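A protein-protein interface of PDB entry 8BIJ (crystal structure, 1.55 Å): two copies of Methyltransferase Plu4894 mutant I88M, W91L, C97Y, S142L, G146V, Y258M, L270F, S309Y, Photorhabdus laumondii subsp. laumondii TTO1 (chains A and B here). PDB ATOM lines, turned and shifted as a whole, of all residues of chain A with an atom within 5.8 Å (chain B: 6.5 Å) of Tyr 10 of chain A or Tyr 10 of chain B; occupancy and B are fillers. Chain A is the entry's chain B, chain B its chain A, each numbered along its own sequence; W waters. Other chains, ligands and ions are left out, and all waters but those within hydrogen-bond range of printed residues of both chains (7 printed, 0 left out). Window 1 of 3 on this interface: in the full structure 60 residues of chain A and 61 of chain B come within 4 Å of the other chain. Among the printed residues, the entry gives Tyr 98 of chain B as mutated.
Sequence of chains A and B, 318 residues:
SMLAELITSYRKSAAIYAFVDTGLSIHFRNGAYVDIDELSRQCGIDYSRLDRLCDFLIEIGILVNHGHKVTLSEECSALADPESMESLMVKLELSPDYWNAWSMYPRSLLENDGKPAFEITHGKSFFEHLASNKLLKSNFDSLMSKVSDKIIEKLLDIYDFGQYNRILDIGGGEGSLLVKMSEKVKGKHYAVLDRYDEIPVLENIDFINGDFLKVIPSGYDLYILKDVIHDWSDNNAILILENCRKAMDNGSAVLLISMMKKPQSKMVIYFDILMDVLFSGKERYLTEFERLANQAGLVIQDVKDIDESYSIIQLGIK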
ATOM      1  N   LEU A   6     -18.794 -11.637 -20.977  1.00  0.00           N
ATOM      2  CA  LEU A   6     -19.300 -12.373 -22.166  1.00  0.00           C
ATOM      3  C   LEU A   6     -18.200 -12.419 -23.232  1.00  0.00           C
ATOM      4  O   LEU A   6     -17.955 -13.504 -23.780  1.00  0.00           O
ATOM      5  CB  LEU A   6     -20.577 -11.709 -22.690  1.00  0.00           C
ATOM      6  CG  LEU A   6     -21.844 -11.981 -21.879  1.00  0.00           C
ATOM      7  CD1 LEU A   6     -23.012 -11.174 -22.422  1.00  0.00           C
ATOM      8  CD2 LEU A   6     -22.190 -13.462 -21.870  1.00  0.00           C
ATOM      9  N   ILE A   7     -17.524 -11.302 -23.496  1.00  0.00           N
ATOM     10  CA  ILE A   7     -16.487 -11.230 -24.568  1.00  0.00           C
ATOM     11  C   ILE A   7     -15.352 -12.216 -24.247  1.00  0.00           C
ATOM     12  O   ILE A   7     -14.875 -12.878 -25.192  1.00  0.00           O
ATOM     13  CB  ILE A   7     -15.977  -9.791 -24.764  1.00  0.00           C
ATOM     14  CG1 ILE A   7     -17.084  -8.871 -25.290  1.00  0.00           C
ATOM     15  CG2 ILE A   7     -14.752  -9.771 -25.671  1.00  0.00           C
ATOM     16  CD1 ILE A   7     -16.774  -7.396 -25.168  1.00  0.00           C
ATOM     17  N   THR A   8     -14.926 -12.304 -22.979  1.00  0.00           N
ATOM     18  CA  THR A   8     -13.718 -13.066 -22.556  1.00  0.00           C
ATOM     19  C   THR A   8     -14.078 -14.499 -22.139  1.00  0.00           C
ATOM     20  O   THR A   8     -13.151 -15.226 -21.740  1.00  0.00           O
ATOM     21  CB  THR A   8     -12.963 -12.335 -21.440  1.00  0.00           C
ATOM     22  OG1 THR A   8     -13.825 -12.220 -20.305  1.00  0.00           O
ATOM     23  CG2 THR A   8     -12.471 -10.977 -21.888  1.00  0.00           C
ATOM     24  N   SER A   9     -15.352 -14.892 -22.258  1.00  0.00           N
ATOM     25  CA  SER A   9     -15.877 -16.240 -21.909  1.00  0.00           C
ATOM     26  C   SER A   9     -14.956 -17.342 -22.454  1.00  0.00           C
ATOM     27  O   SER A   9     -14.672 -18.305 -21.708  1.00  0.00           O
ATOM     28  CB  SER A   9     -17.280 -16.416 -22.435  1.00  0.00           C
ATOM     29  OG  SER A   9     -18.222 -15.742 -21.622  1.00  0.00           O
ATOM     30  N   TYR A  10     -14.533 -17.222 -23.715  1.00  0.00           N
ATOM     31  CA  TYR A  10     -13.744 -18.242 -24.457  1.00  0.00           C
ATOM     32  C   TYR A  10     -12.482 -18.626 -23.675  1.00  0.00           C
ATOM     33  O   TYR A  10     -12.021 -19.760 -23.797  1.00  0.00           O
ATOM     34  CB  TYR A  10     -13.392 -17.743 -25.860  1.00  0.00           C
ATOM     35  CG  TYR A  10     -12.310 -16.695 -25.871  1.00  0.00           C
ATOM     36  CD1 TYR A  10     -12.613 -15.368 -25.614  1.00  0.00           C
ATOM     37  CD2 TYR A  10     -10.986 -17.031 -26.091  1.00  0.00           C
ATOM     38  CE1 TYR A  10     -11.623 -14.396 -25.587  1.00  0.00           C
ATOM     39  CE2 TYR A  10      -9.984 -16.068 -26.068  1.00  0.00           C
ATOM     40  CZ  TYR A  10     -10.305 -14.744 -25.821  1.00  0.00           C
ATOM     41  OH  TYR A  10      -9.317 -13.794 -25.800  1.00  0.00           O
ATOM     42  N   ARG A  11     -11.901 -17.694 -22.908  1.00  0.00           N
ATOM     43  CA  ARG A  11     -10.663 -17.974 -22.129  1.00  0.00           C
ATOM     44  C   ARG A  11     -10.938 -19.071 -21.090  1.00  0.00           C
ATOM     45  O   ARG A  11     -10.020 -19.865 -20.820  1.00  0.00           O
ATOM     46  CB  ARG A  11     -10.124 -16.695 -21.482  1.00  0.00           C
ATOM     47  CG  ARG A  11      -9.693 -15.645 -22.494  1.00  0.00           C
ATOM     48  CD  ARG A  11      -8.928 -14.512 -21.854  1.00  0.00           C
ATOM     49  NE  ARG A  11      -8.975 -13.332 -22.702  1.00  0.00           N
ATOM     50  CZ  ARG A  11      -8.817 -12.090 -22.267  1.00  0.00           C
ATOM     51  NH1 ARG A  11      -8.585 -11.864 -20.987  1.00  0.00           N
ATOM     52  NH2 ARG A  11      -8.913 -11.081 -23.108  1.00  0.00           N
ATOM     53  N   LYS A  12     -12.152 -19.116 -20.533  1.00  0.00           N
ATOM     54  CA  LYS A  12     -12.557 -20.144 -19.538  1.00  0.00           C
ATOM     55  C   LYS A  12     -12.510 -21.522 -20.211  1.00  0.00           C
ATOM     56  O   LYS A  12     -11.924 -22.452 -19.633  1.00  0.00           O
ATOM     57  CB  LYS A  12     -13.976 -19.909 -19.016  1.00  0.00           C
ATOM     58  CG  LYS A  12     -14.248 -18.588 -18.320  1.00  0.00           C
ATOM     59  CD  LYS A  12     -15.736 -18.398 -18.097  1.00  0.00           C
ATOM     60  CE  LYS A  12     -16.070 -17.368 -17.045  1.00  0.00           C
ATOM     61  NZ  LYS A  12     -17.482 -17.479 -16.612  1.00  0.00           N
ATOM     62  N   SER A  13     -13.089 -21.636 -21.403  1.00  0.00           N
ATOM     63  CA  SER A  13     -13.143 -22.919 -22.154  1.00  0.00           C
ATOM     64  C   SER A  13     -11.713 -23.350 -22.499  1.00  0.00           C
ATOM     65  O   SER A  13     -11.356 -24.508 -22.249  1.00  0.00           O
ATOM     66  CB  SER A  13     -14.013 -22.817 -23.378  1.00  0.00           C
ATOM     67  OG  SER A  13     -15.277 -22.265 -23.051  1.00  0.00           O
ATOM     68  N   ALA A  14     -10.884 -22.419 -22.980  1.00  0.00           N
ATOM     69  CA  ALA A  14      -9.493 -22.718 -23.389  1.00  0.00           C
ATOM     70  C   ALA A  14      -8.689 -23.217 -22.178  1.00  0.00           C
ATOM     71  O   ALA A  14      -7.905 -24.165 -22.344  1.00  0.00           O
ATOM     72  CB  ALA A  14      -8.869 -21.498 -24.017  1.00  0.00           C
ATOM     73  N   ALA A  15      -8.858 -22.590 -21.004  1.00  0.00           N
ATOM     74  CA  ALA A  15      -8.131 -22.958 -19.764  1.00  0.00           C
ATOM     75  C   ALA A  15      -8.510 -24.387 -19.332  1.00  0.00           C
ATOM     76  O   ALA A  15      -7.619 -25.126 -18.892  1.00  0.00           O
ATOM     77  CB  ALA A  15      -8.408 -21.957 -18.670  1.00  0.00           C
ATOM     78  N   GLU A  93     -14.877 -31.032 -28.580  1.00  0.00           N
ATOM     79  CA  GLU A  93     -15.351 -29.736 -29.138  1.00  0.00           C
ATOM     80  C   GLU A  93     -14.343 -28.616 -28.860  1.00  0.00           C
ATOM     81  O   GLU A  93     -14.442 -27.575 -29.545  1.00  0.00           O
ATOM     82  CB  GLU A  93     -16.754 -29.383 -28.642  1.00  0.00           C
ATOM     83  CG  GLU A  93     -16.827 -28.772 -27.258  1.00  0.00           C
ATOM     84  CD  GLU A  93     -18.261 -28.470 -26.862  1.00  0.00           C
ATOM     85  OE1 GLU A  93     -18.972 -29.418 -26.438  1.00  0.00           O
ATOM     86  OE2 GLU A  93     -18.690 -27.310 -27.054  1.00  0.00           O
ATOM     87  N   LEU A  94     -13.407 -28.794 -27.920  1.00  0.00           N
ATOM     88  CA  LEU A  94     -12.367 -27.761 -27.651  1.00  0.00           C
ATOM     89  C   LEU A  94     -11.034 -28.145 -28.308  1.00  0.00           C
ATOM     90  O   LEU A  94     -10.067 -27.389 -28.129  1.00  0.00           O
ATOM     91  CB  LEU A  94     -12.208 -27.546 -26.143  1.00  0.00           C
ATOM     92  CG  LEU A  94     -13.455 -27.082 -25.396  1.00  0.00           C
ATOM     93  CD1 LEU A  94     -13.154 -26.850 -23.926  1.00  0.00           C
ATOM     94  CD2 LEU A  94     -14.075 -25.843 -26.024  1.00  0.00           C
ATOM     95  N   TRP A  99     -12.198 -25.850 -32.508  1.00  0.00           N
ATOM     96  CA  TRP A  99     -11.929 -24.487 -31.977  1.00  0.00           C
ATOM     97  C   TRP A  99     -11.668 -23.515 -33.131  1.00  0.00           C
ATOM     98  O   TRP A  99     -12.311 -22.440 -33.175  1.00  0.00           O
ATOM     99  CB  TRP A  99     -10.751 -24.553 -31.005  1.00  0.00           C
ATOM    100  CG  TRP A  99     -10.394 -23.232 -30.404  1.00  0.00           C
ATOM    101  CD1 TRP A  99      -9.499 -22.325 -30.886  1.00  0.00           C
ATOM    102  CD2 TRP A  99     -10.926 -22.681 -29.191  1.00  0.00           C
ATOM    103  NE1 TRP A  99      -9.436 -21.247 -30.051  1.00  0.00           N
ATOM    104  CE2 TRP A  99     -10.295 -21.432 -29.001  1.00  0.00           C
ATOM    105  CE3 TRP A  99     -11.861 -23.116 -28.247  1.00  0.00           C
ATOM    106  CZ2 TRP A  99     -10.583 -20.620 -27.907  1.00  0.00           C
ATOM    107  CZ3 TRP A  99     -12.142 -22.316 -27.162  1.00  0.00           C
ATOM    108  CH2 TRP A  99     -11.508 -21.085 -26.997  1.00  0.00           C
ATOM    109  N   TRP A 102     -14.455 -21.768 -35.460  1.00  0.00           N
ATOM    110  CA  TRP A 102     -15.368 -20.728 -34.916  1.00  0.00           C
ATOM    111  C   TRP A 102     -14.955 -19.331 -35.381  1.00  0.00           C
ATOM    112  O   TRP A 102     -15.857 -18.498 -35.548  1.00  0.00           O
ATOM    113  CB  TRP A 102     -15.441 -20.795 -33.391  1.00  0.00           C
ATOM    114  CG  TRP A 102     -16.275 -21.947 -32.942  1.00  0.00           C
ATOM    115  CD1 TRP A 102     -15.852 -23.224 -32.747  1.00  0.00           C
ATOM    116  CD2 TRP A 102     -17.686 -21.931 -32.679  1.00  0.00           C
ATOM    117  NE1 TRP A 102     -16.906 -24.012 -32.373  1.00  0.00           N
ATOM    118  CE2 TRP A 102     -18.042 -23.249 -32.325  1.00  0.00           C
ATOM    119  CE3 TRP A 102     -18.681 -20.950 -32.713  1.00  0.00           C
ATOM    120  CZ2 TRP A 102     -19.349 -23.591 -31.981  1.00  0.00           C
ATOM    121  CZ3 TRP A 102     -19.970 -21.291 -32.369  1.00  0.00           C
ATOM    122  CH2 TRP A 102     -20.297 -22.598 -32.016  1.00  0.00           C
ATOM    123  N   TYR A 270     -28.483 -23.204 -27.858  1.00  0.00           N
ATOM    124  CA  TYR A 270     -27.034 -23.136 -27.557  1.00  0.00           C
ATOM    125  C   TYR A 270     -26.263 -24.096 -28.476  1.00  0.00           C
ATOM    126  O   TYR A 270     -25.187 -23.727 -28.958  1.00  0.00           O
ATOM    127  CB  TYR A 270     -26.809 -23.394 -26.066  1.00  0.00           C
ATOM    128  CG  TYR A 270     -25.571 -22.726 -25.547  1.00  0.00           C
ATOM    129  CD1 TYR A 270     -25.587 -21.399 -25.141  1.00  0.00           C
ATOM    130  CD2 TYR A 270     -24.363 -23.398 -25.537  1.00  0.00           C
ATOM    131  CE1 TYR A 270     -24.438 -20.769 -24.696  1.00  0.00           C
ATOM    132  CE2 TYR A 270     -23.206 -22.780 -25.101  1.00  0.00           C
ATOM    133  CZ  TYR A 270     -23.242 -21.465 -24.677  1.00  0.00           C
ATOM    134  OH  TYR A 270     -22.084 -20.879 -24.256  1.00  0.00           O
ATOM    135  N   LEU A 274     -23.401 -24.470 -33.017  1.00  0.00           N
ATOM    136  CA  LEU A 274     -22.325 -25.460 -33.289  1.00  0.00           C
ATOM    137  C   LEU A 274     -22.649 -26.231 -34.575  1.00  0.00           C
ATOM    138  O   LEU A 274     -21.720 -26.493 -35.352  1.00  0.00           O
ATOM    139  CB  LEU A 274     -22.190 -26.407 -32.095  1.00  0.00           C
ATOM    140  CG  LEU A 274     -21.104 -27.476 -32.200  1.00  0.00           C
ATOM    141  CD1 LEU A 274     -19.792 -26.902 -32.699  1.00  0.00           C
ATOM    142  CD2 LEU A 274     -20.892 -28.151 -30.854  1.00  0.00           C
ATOM    143  N   GLU B   5     -21.551 -25.636 -18.676  1.00  0.00           N
ATOM    144  CA  GLU B   5     -21.730 -24.207 -19.056  1.00  0.00           C
ATOM    145  C   GLU B   5     -20.359 -23.531 -19.197  1.00  0.00           C
ATOM    146  O   GLU B   5     -20.195 -22.750 -20.154  1.00  0.00           O
ATOM    147  CB  GLU B   5     -22.629 -23.490 -18.048  1.00  0.00           C
ATOM    148  CG  GLU B   5     -24.090 -23.894 -18.167  1.00  0.00           C
ATOM    149  CD  GLU B   5     -25.049 -23.170 -17.239  1.00  0.00           C
ATOM    150  OE1 GLU B   5     -24.665 -22.113 -16.694  1.00  0.00           O
ATOM    151  OE2 GLU B   5     -26.184 -23.662 -17.067  1.00  0.00           O
ATOM    152  N   LEU B   6     -19.405 -23.813 -18.303  1.00  0.00           N
ATOM    153  CA  LEU B   6     -18.017 -23.283 -18.427  1.00  0.00           C
ATOM    154  C   LEU B   6     -17.386 -23.852 -19.703  1.00  0.00           C
ATOM    155  O   LEU B   6     -16.777 -23.086 -20.453  1.00  0.00           O
ATOM    156  CB  LEU B   6     -17.188 -23.640 -17.188  1.00  0.00           C
ATOM    157  CG  LEU B   6     -17.514 -22.863 -15.914  1.00  0.00           C
ATOM    158  CD1 LEU B   6     -16.688 -23.374 -14.744  1.00  0.00           C
ATOM    159  CD2 LEU B   6     -17.292 -21.370 -16.097  1.00  0.00           C
ATOM    160  N   ILE B   7     -17.558 -25.148 -19.969  1.00  0.00           N
ATOM    161  CA  ILE B   7     -16.926 -25.822 -21.142  1.00  0.00           C
ATOM    162  C   ILE B   7     -17.398 -25.143 -22.437  1.00  0.00           C
ATOM    163  O   ILE B   7     -16.558 -24.949 -23.333  1.00  0.00           O
ATOM    164  CB  ILE B   7     -17.214 -27.335 -21.133  1.00  0.00           C
ATOM    165  CG1 ILE B   7     -16.475 -28.034 -19.989  1.00  0.00           C
ATOM    166  CG2 ILE B   7     -16.895 -27.970 -22.483  1.00  0.00           C
ATOM    167  CD1 ILE B   7     -17.000 -29.421 -19.678  1.00  0.00           C
ATOM    168  N   THR B   8     -18.686 -24.793 -22.533  1.00  0.00           N
ATOM    169  CA  THR B   8     -19.318 -24.295 -23.786  1.00  0.00           C
ATOM    170  C   THR B   8     -19.329 -22.756 -23.804  1.00  0.00           C
ATOM    171  O   THR B   8     -19.901 -22.206 -24.770  1.00  0.00           O
ATOM    172  CB  THR B   8     -20.707 -24.921 -23.999  1.00  0.00           C
ATOM    173  OG1 THR B   8     -21.599 -24.518 -22.958  1.00  0.00           O
ATOM    174  CG2 THR B   8     -20.679 -26.435 -24.071  1.00  0.00           C
ATOM    175  N   SER B   9     -18.678 -22.096 -22.826  1.00  0.00           N
ATOM    176  CA  SER B   9     -18.624 -20.617 -22.657  1.00  0.00           C
ATOM    177  C   SER B   9     -18.174 -19.944 -23.961  1.00  0.00           C
ATOM    178  O   SER B   9     -18.725 -18.879 -24.295  1.00  0.00           O
ATOM    179  CB  SER B   9     -17.687 -20.208 -21.529  1.00  0.00           C
ATOM    180  OG  SER B   9     -18.255 -20.461 -20.257  1.00  0.00           O
ATOM    181  N   TYR B  10     -17.184 -20.529 -24.640  1.00  0.00           N
ATOM    182  CA  TYR B  10     -16.509 -19.964 -25.842  1.00  0.00           C
ATOM    183  C   TYR B  10     -17.535 -19.602 -26.925  1.00  0.00           C
ATOM    184  O   TYR B  10     -17.274 -18.684 -27.708  1.00  0.00           O
ATOM    185  CB  TYR B  10     -15.466 -20.940 -26.395  1.00  0.00           C
ATOM    186  CG  TYR B  10     -16.086 -22.155 -27.033  1.00  0.00           C
ATOM    187  CD1 TYR B  10     -16.483 -23.235 -26.261  1.00  0.00           C
ATOM    188  CD2 TYR B  10     -16.339 -22.203 -28.395  1.00  0.00           C
ATOM    189  CE1 TYR B  10     -17.100 -24.336 -26.833  1.00  0.00           C
ATOM    190  CE2 TYR B  10     -16.947 -23.306 -28.982  1.00  0.00           C
ATOM    191  CZ  TYR B  10     -17.323 -24.378 -28.195  1.00  0.00           C
ATOM    192  OH  TYR B  10     -17.950 -25.483 -28.729  1.00  0.00           O
ATOM    193  N   ARG B  11     -18.670 -20.303 -26.999  1.00  0.00           N
ATOM    194  CA  ARG B  11     -19.688 -20.048 -28.054  1.00  0.00           C
ATOM    195  C   ARG B  11     -20.250 -18.630 -27.900  1.00  0.00           C
ATOM    196  O   ARG B  11     -20.586 -18.015 -28.929  1.00  0.00           O
ATOM    197  CB  ARG B  11     -20.808 -21.095 -28.013  1.00  0.00           C
ATOM    198  CG  ARG B  11     -20.320 -22.514 -28.260  1.00  0.00           C
ATOM    199  CD  ARG B  11     -21.478 -23.474 -28.429  1.00  0.00           C
ATOM    200  NE  ARG B  11     -21.054 -24.848 -28.197  1.00  0.00           N
ATOM    201  CZ  ARG B  11     -21.862 -25.848 -27.866  1.00  0.00           C
ATOM    202  NH1 ARG B  11     -23.164 -25.654 -27.755  1.00  0.00           N
ATOM    203  NH2 ARG B  11     -21.357 -27.049 -27.653  1.00  0.00           N
ATOM    204  N   LYS B  12     -20.349 -18.134 -26.662  1.00  0.00           N
ATOM    205  CA  LYS B  12     -20.841 -16.767 -26.351  1.00  0.00           C
ATOM    206  C   LYS B  12     -19.917 -15.758 -27.049  1.00  0.00           C
ATOM    207  O   LYS B  12     -20.413 -14.909 -27.815  1.00  0.00           O
ATOM    208  CB  LYS B  12     -20.879 -16.537 -24.836  1.00  0.00           C
ATOM    209  CG  LYS B  12     -21.827 -17.434 -24.048  1.00  0.00           C
ATOM    210  CD  LYS B  12     -21.681 -17.265 -22.550  1.00  0.00           C
ATOM    211  CE  LYS B  12     -22.559 -18.184 -21.728  1.00  0.00           C
ATOM    212  NZ  LYS B  12     -22.473 -17.844 -20.289  1.00  0.00           N
ATOM    213  N   SER B  13     -18.610 -15.889 -26.833  1.00  0.00           N
ATOM    214  CA  SER B  13     -17.580 -14.999 -27.427  1.00  0.00           C
ATOM    215  C   SER B  13     -17.698 -15.033 -28.954  1.00  0.00           C
ATOM    216  O   SER B  13     -17.790 -13.970 -29.574  1.00  0.00           O
ATOM    217  CB  SER B  13     -16.202 -15.386 -26.965  1.00  0.00           C
ATOM    218  OG  SER B  13     -16.134 -15.396 -25.548  1.00  0.00           O
ATOM    219  N   ALA B  14     -17.768 -16.231 -29.543  1.00  0.00           N
ATOM    220  CA  ALA B  14     -17.803 -16.412 -31.011  1.00  0.00           C
ATOM    221  C   ALA B  14     -19.070 -15.770 -31.594  1.00  0.00           C
ATOM    222  O   ALA B  14     -18.979 -15.189 -32.683  1.00  0.00           O
ATOM    223  CB  ALA B  14     -17.712 -17.878 -31.357  1.00  0.00           C
ATOM    224  N   ALA B  15     -20.218 -15.889 -30.917  1.00  0.00           N
ATOM    225  CA  ALA B  15     -21.500 -15.288 -31.362  1.00  0.00           C
ATOM    226  C   ALA B  15     -21.377 -13.758 -31.361  1.00  0.00           C
ATOM    227  O   ALA B  15     -21.869 -13.113 -32.305  1.00  0.00           O
ATOM    228  CB  ALA B  15     -22.638 -15.749 -30.484  1.00  0.00           C
ATOM    229  N   GLU B  93      -9.285  -9.667 -30.721  1.00  0.00           N
ATOM    230  CA  GLU B  93      -9.126 -10.786 -29.753  1.00  0.00           C
ATOM    231  C   GLU B  93      -9.781 -12.072 -30.280  1.00  0.00           C
ATOM    232  O   GLU B  93      -9.253 -13.174 -30.003  1.00  0.00           O
ATOM    233  CB  GLU B  93      -9.799 -10.335 -28.460  1.00  0.00           C
ATOM    234  CG  GLU B  93      -9.343 -11.052 -27.227  1.00  0.00           C
ATOM    235  CD  GLU B  93     -10.228 -10.741 -26.036  1.00  0.00           C
ATOM    236  OE1 GLU B  93     -10.853  -9.650 -26.008  1.00  0.00           O
ATOM    237  OE2 GLU B  93     -10.247 -11.556 -25.124  1.00  0.00           O
ATOM    238  N   LEU B  94     -10.898 -11.947 -30.997  1.00  0.00           N
ATOM    239  CA  LEU B  94     -11.719 -13.108 -31.433  1.00  0.00           C
ATOM    240  C   LEU B  94     -11.474 -13.401 -32.919  1.00  0.00           C
ATOM    241  O   LEU B  94     -12.056 -14.360 -33.416  1.00  0.00           O
ATOM    242  CB  LEU B  94     -13.191 -12.815 -31.128  1.00  0.00           C
ATOM    243  CG  LEU B  94     -13.485 -12.362 -29.697  1.00  0.00           C
ATOM    244  CD1 LEU B  94     -14.971 -12.135 -29.486  1.00  0.00           C
ATOM    245  CD2 LEU B  94     -12.950 -13.355 -28.673  1.00  0.00           C
ATOM    246  N   TYR B  98      -5.610 -14.492 -33.531  1.00  0.00           N
ATOM    247  CA  TYR B  98      -5.524 -14.460 -32.048  1.00  0.00           C
ATOM    248  C   TYR B  98      -6.333 -15.631 -31.464  1.00  0.00           C
ATOM    249  O   TYR B  98      -5.759 -16.423 -30.694  1.00  0.00           O
ATOM    250  CB  TYR B  98      -5.900 -13.048 -31.600  1.00  0.00           C
ATOM    251  CG  TYR B  98      -5.068 -11.995 -32.300  1.00  0.00           C
ATOM    252  CD1 TYR B  98      -3.730 -11.805 -31.985  1.00  0.00           C
ATOM    253  CD2 TYR B  98      -5.570 -11.269 -33.368  1.00  0.00           C
ATOM    254  CE1 TYR B  98      -2.945 -10.876 -32.657  1.00  0.00           C
ATOM    255  CE2 TYR B  98      -4.802 -10.325 -34.043  1.00  0.00           C
ATOM    256  CZ  TYR B  98      -3.475 -10.132 -33.696  1.00  0.00           C
ATOM    257  OH  TYR B  98      -2.698  -9.206 -34.354  1.00  0.00           O
ATOM    258  N   TRP B  99      -7.611 -15.733 -31.826  1.00  0.00           N
ATOM    259  CA  TRP B  99      -8.480 -16.876 -31.430  1.00  0.00           C
ATOM    260  C   TRP B  99      -7.733 -18.202 -31.632  1.00  0.00           C
ATOM    261  O   TRP B  99      -7.695 -19.014 -30.676  1.00  0.00           O
ATOM    262  CB  TRP B  99      -9.804 -16.841 -32.199  1.00  0.00           C
ATOM    263  CG  TRP B  99     -10.743 -17.977 -31.889  1.00  0.00           C
ATOM    264  CD1 TRP B  99     -10.746 -19.225 -32.437  1.00  0.00           C
ATOM    265  CD2 TRP B  99     -11.831 -17.953 -30.951  1.00  0.00           C
ATOM    266  NE1 TRP B  99     -11.766 -19.974 -31.912  1.00  0.00           N
ATOM    267  CE2 TRP B  99     -12.455 -19.224 -31.000  1.00  0.00           C
ATOM    268  CE3 TRP B  99     -12.351 -16.989 -30.083  1.00  0.00           C
ATOM    269  CZ2 TRP B  99     -13.548 -19.538 -30.200  1.00  0.00           C
ATOM    270  CZ3 TRP B  99     -13.434 -17.299 -29.296  1.00  0.00           C
ATOM    271  CH2 TRP B  99     -14.032 -18.558 -29.368  1.00  0.00           C
ATOM    272  N   TRP B 102      -4.858 -19.849 -29.256  1.00  0.00           N
ATOM    273  CA  TRP B 102      -5.250 -20.555 -28.009  1.00  0.00           C
ATOM    274  C   TRP B 102      -5.178 -22.074 -28.217  1.00  0.00           C
ATOM    275  O   TRP B 102      -4.966 -22.786 -27.219  1.00  0.00           O
ATOM    276  CB  TRP B 102      -6.628 -20.088 -27.538  1.00  0.00           C
ATOM    277  CG  TRP B 102      -6.603 -18.698 -26.991  1.00  0.00           C
ATOM    278  CD1 TRP B 102      -6.666 -17.536 -27.695  1.00  0.00           C
ATOM    279  CD2 TRP B 102      -6.503 -18.332 -25.607  1.00  0.00           C
ATOM    280  NE1 TRP B 102      -6.586 -16.464 -26.846  1.00  0.00           N
ATOM    281  CE2 TRP B 102      -6.484 -16.921 -25.558  1.00  0.00           C
ATOM    282  CE3 TRP B 102      -6.395 -19.054 -24.414  1.00  0.00           C
ATOM    283  CZ2 TRP B 102      -6.413 -16.231 -24.352  1.00  0.00           C
ATOM    284  CZ3 TRP B 102      -6.320 -18.369 -23.223  1.00  0.00           C
ATOM    285  CH2 TRP B 102      -6.322 -16.974 -23.197  1.00  0.00           C
ATOM    286  N   LEU B 274      -4.058 -14.296 -21.200  1.00  0.00           N
ATOM    287  CA  LEU B 274      -3.910 -13.750 -22.577  1.00  0.00           C
ATOM    288  C   LEU B 274      -2.449 -13.330 -22.805  1.00  0.00           C
ATOM    289  O   LEU B 274      -1.915 -13.572 -23.903  1.00  0.00           O
ATOM    290  CB  LEU B 274      -4.860 -12.571 -22.790  1.00  0.00           C
ATOM    291  CG  LEU B 274      -4.768 -11.903 -24.162  1.00  0.00           C
ATOM    292  CD1 LEU B 274      -5.239 -12.843 -25.263  1.00  0.00           C
ATOM    293  CD2 LEU B 274      -5.558 -10.602 -24.185  1.00  0.00           C
HETATM  294  O   HOH W   1     -16.557 -26.531 -30.884  1.00  0.00           O
HETATM  295  O   HOH W   2     -21.913 -22.090 -21.946  1.00  0.00           O
HETATM  296  O   HOH W   3     -19.533 -16.416 -19.472  1.00  0.00           O
HETATM  297  O   HOH W   4      -9.488  -8.393 -23.238  1.00  0.00           O
HETATM  298  O   HOH W   5     -21.490 -29.975 -26.756  1.00  0.00           O
HETATM  299  O   HOH W   6      -5.927 -24.341 -24.255  1.00  0.00           O
HETATM  300  O   HOH W   7      -7.525 -13.925 -27.966  1.00  0.00           O
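The side-chain hydroxyl (OG) of Ser 9 of chain B is in hydrogen-bond range of the backbone carbonyl oxygen (O) of Leu 6 of chain B.
NE of Arg 11 of chain A sits at hydrogen-bond distance from OH of Tyr 10 of chain A, 3.2 Å away.
The side-chain hydroxyl (OG) of Ser 13 of chain A sits at hydrogen-bond distance from the backbone carbonyl oxygen (O) of Ile 7 of chain B (3.0 Å).
The side-chain hydroxyl of Tyr 270 of chain A is in hydrogen-bond range of the backbone carbonyl oxygen of Thr 8 of chain B (2.6 Å).
The backbone NH of Ser 9 of chain B sits at hydrogen-bond distance from the side-chain hydroxyl of Ser 13 of chain A, 3.4 Å away.
OG of Ser 13 of chain A is in hydrogen-bond range of N of Tyr 10 of chain B (3.0 Å).
OE2 of Glu 93 of chain A lies within hydrogen-bond range of OH of Tyr 10 of chain B (2.6 Å).
OE2 of Glu 93 of chain A lies within salt-bridge range of NH2 of Arg 11 of chain B.
NH1 of Arg 11 of chain B is in hydrogen-bond range of O of Tyr 270 of chain A (3.0 Å).
OG of Ser 13 of chain B sits at hydrogen-bond distance from O of Leu 6 of chain A (3.2 Å).
The side-chain hydroxyl (OG) of Ser 13 of chain B is in hydrogen-bond range of the backbone carbonyl oxygen (O) of Ile 7 of chain A, 2.8 Å away.
The backbone NH (N) of Ser 9 of chain A sits at hydrogen-bond distance from the side-chain hydroxyl (OG) of Ser 13 of chain B (3.4 Å).
The side-chain hydroxyl of Ser 13 of chain B lies within hydrogen-bond range of the backbone NH of Tyr 10 of chain A.
The side-chain carboxylate of Glu 93 of chain B is in hydrogen-bond range of the side-chain hydroxyl of Tyr 10 of chain A (2.5 Å).
The side-chain carboxylate (OE2) of Glu 93 of chain B lies within salt-bridge range of the guanidinium group (NH2) of Arg 11 of chain A (2.5 Å).
Tyr 10 of chain A touches Tyr 10 of chain B.
CB of Trp 102 of chain A touches CZ2 of Trp 99 of chain B, 3.9 Å away.
Ser 9 of chain B touches Tyr 270 of chain A.
Tyr 270 of chain A touches Lys 12 of chain B.
Tyr 10 of chain A touches Ser 13 of chain B, and with the chains exchanged Ser 13 of chain A touches Tyr 10 of chain B.
Tyr 10 of chain A touches Leu 94 of chain B, and with the chains exchanged Leu 94 of chain A touches Tyr 10 of chain B.
Of the 16 printed residues of chain A, 15 touch a printed residue of chain B.
Of chain B, only Tyr 10, Ser 13, Glu 93, Leu 94, Trp 99 and Trp 102 come within 4 Å of Tyr 10 of chain A.
Tyr 10 of chain B touches just these residues of chain A: Tyr 10, Ser 13, Glu 93, Leu 94, Trp 99 and Trp 102.
Of the printed residues of chain A, Leu 6 of chain B touches Lys 12 and Ser 13.
Printed residues of chain B within 4 Å of Ile 7 of chain A: Ser 13 (2.8 Å) and Glu 93 (3.9 Å).
The nearest printed residue of chain A that does not touch Tyr 10 of chain B is Ser 9 of chain A (4.5 Å).
The nearest printed residue of chain B that does not touch Leu 274 of chain A is Tyr 10 of chain B (4.5 Å).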
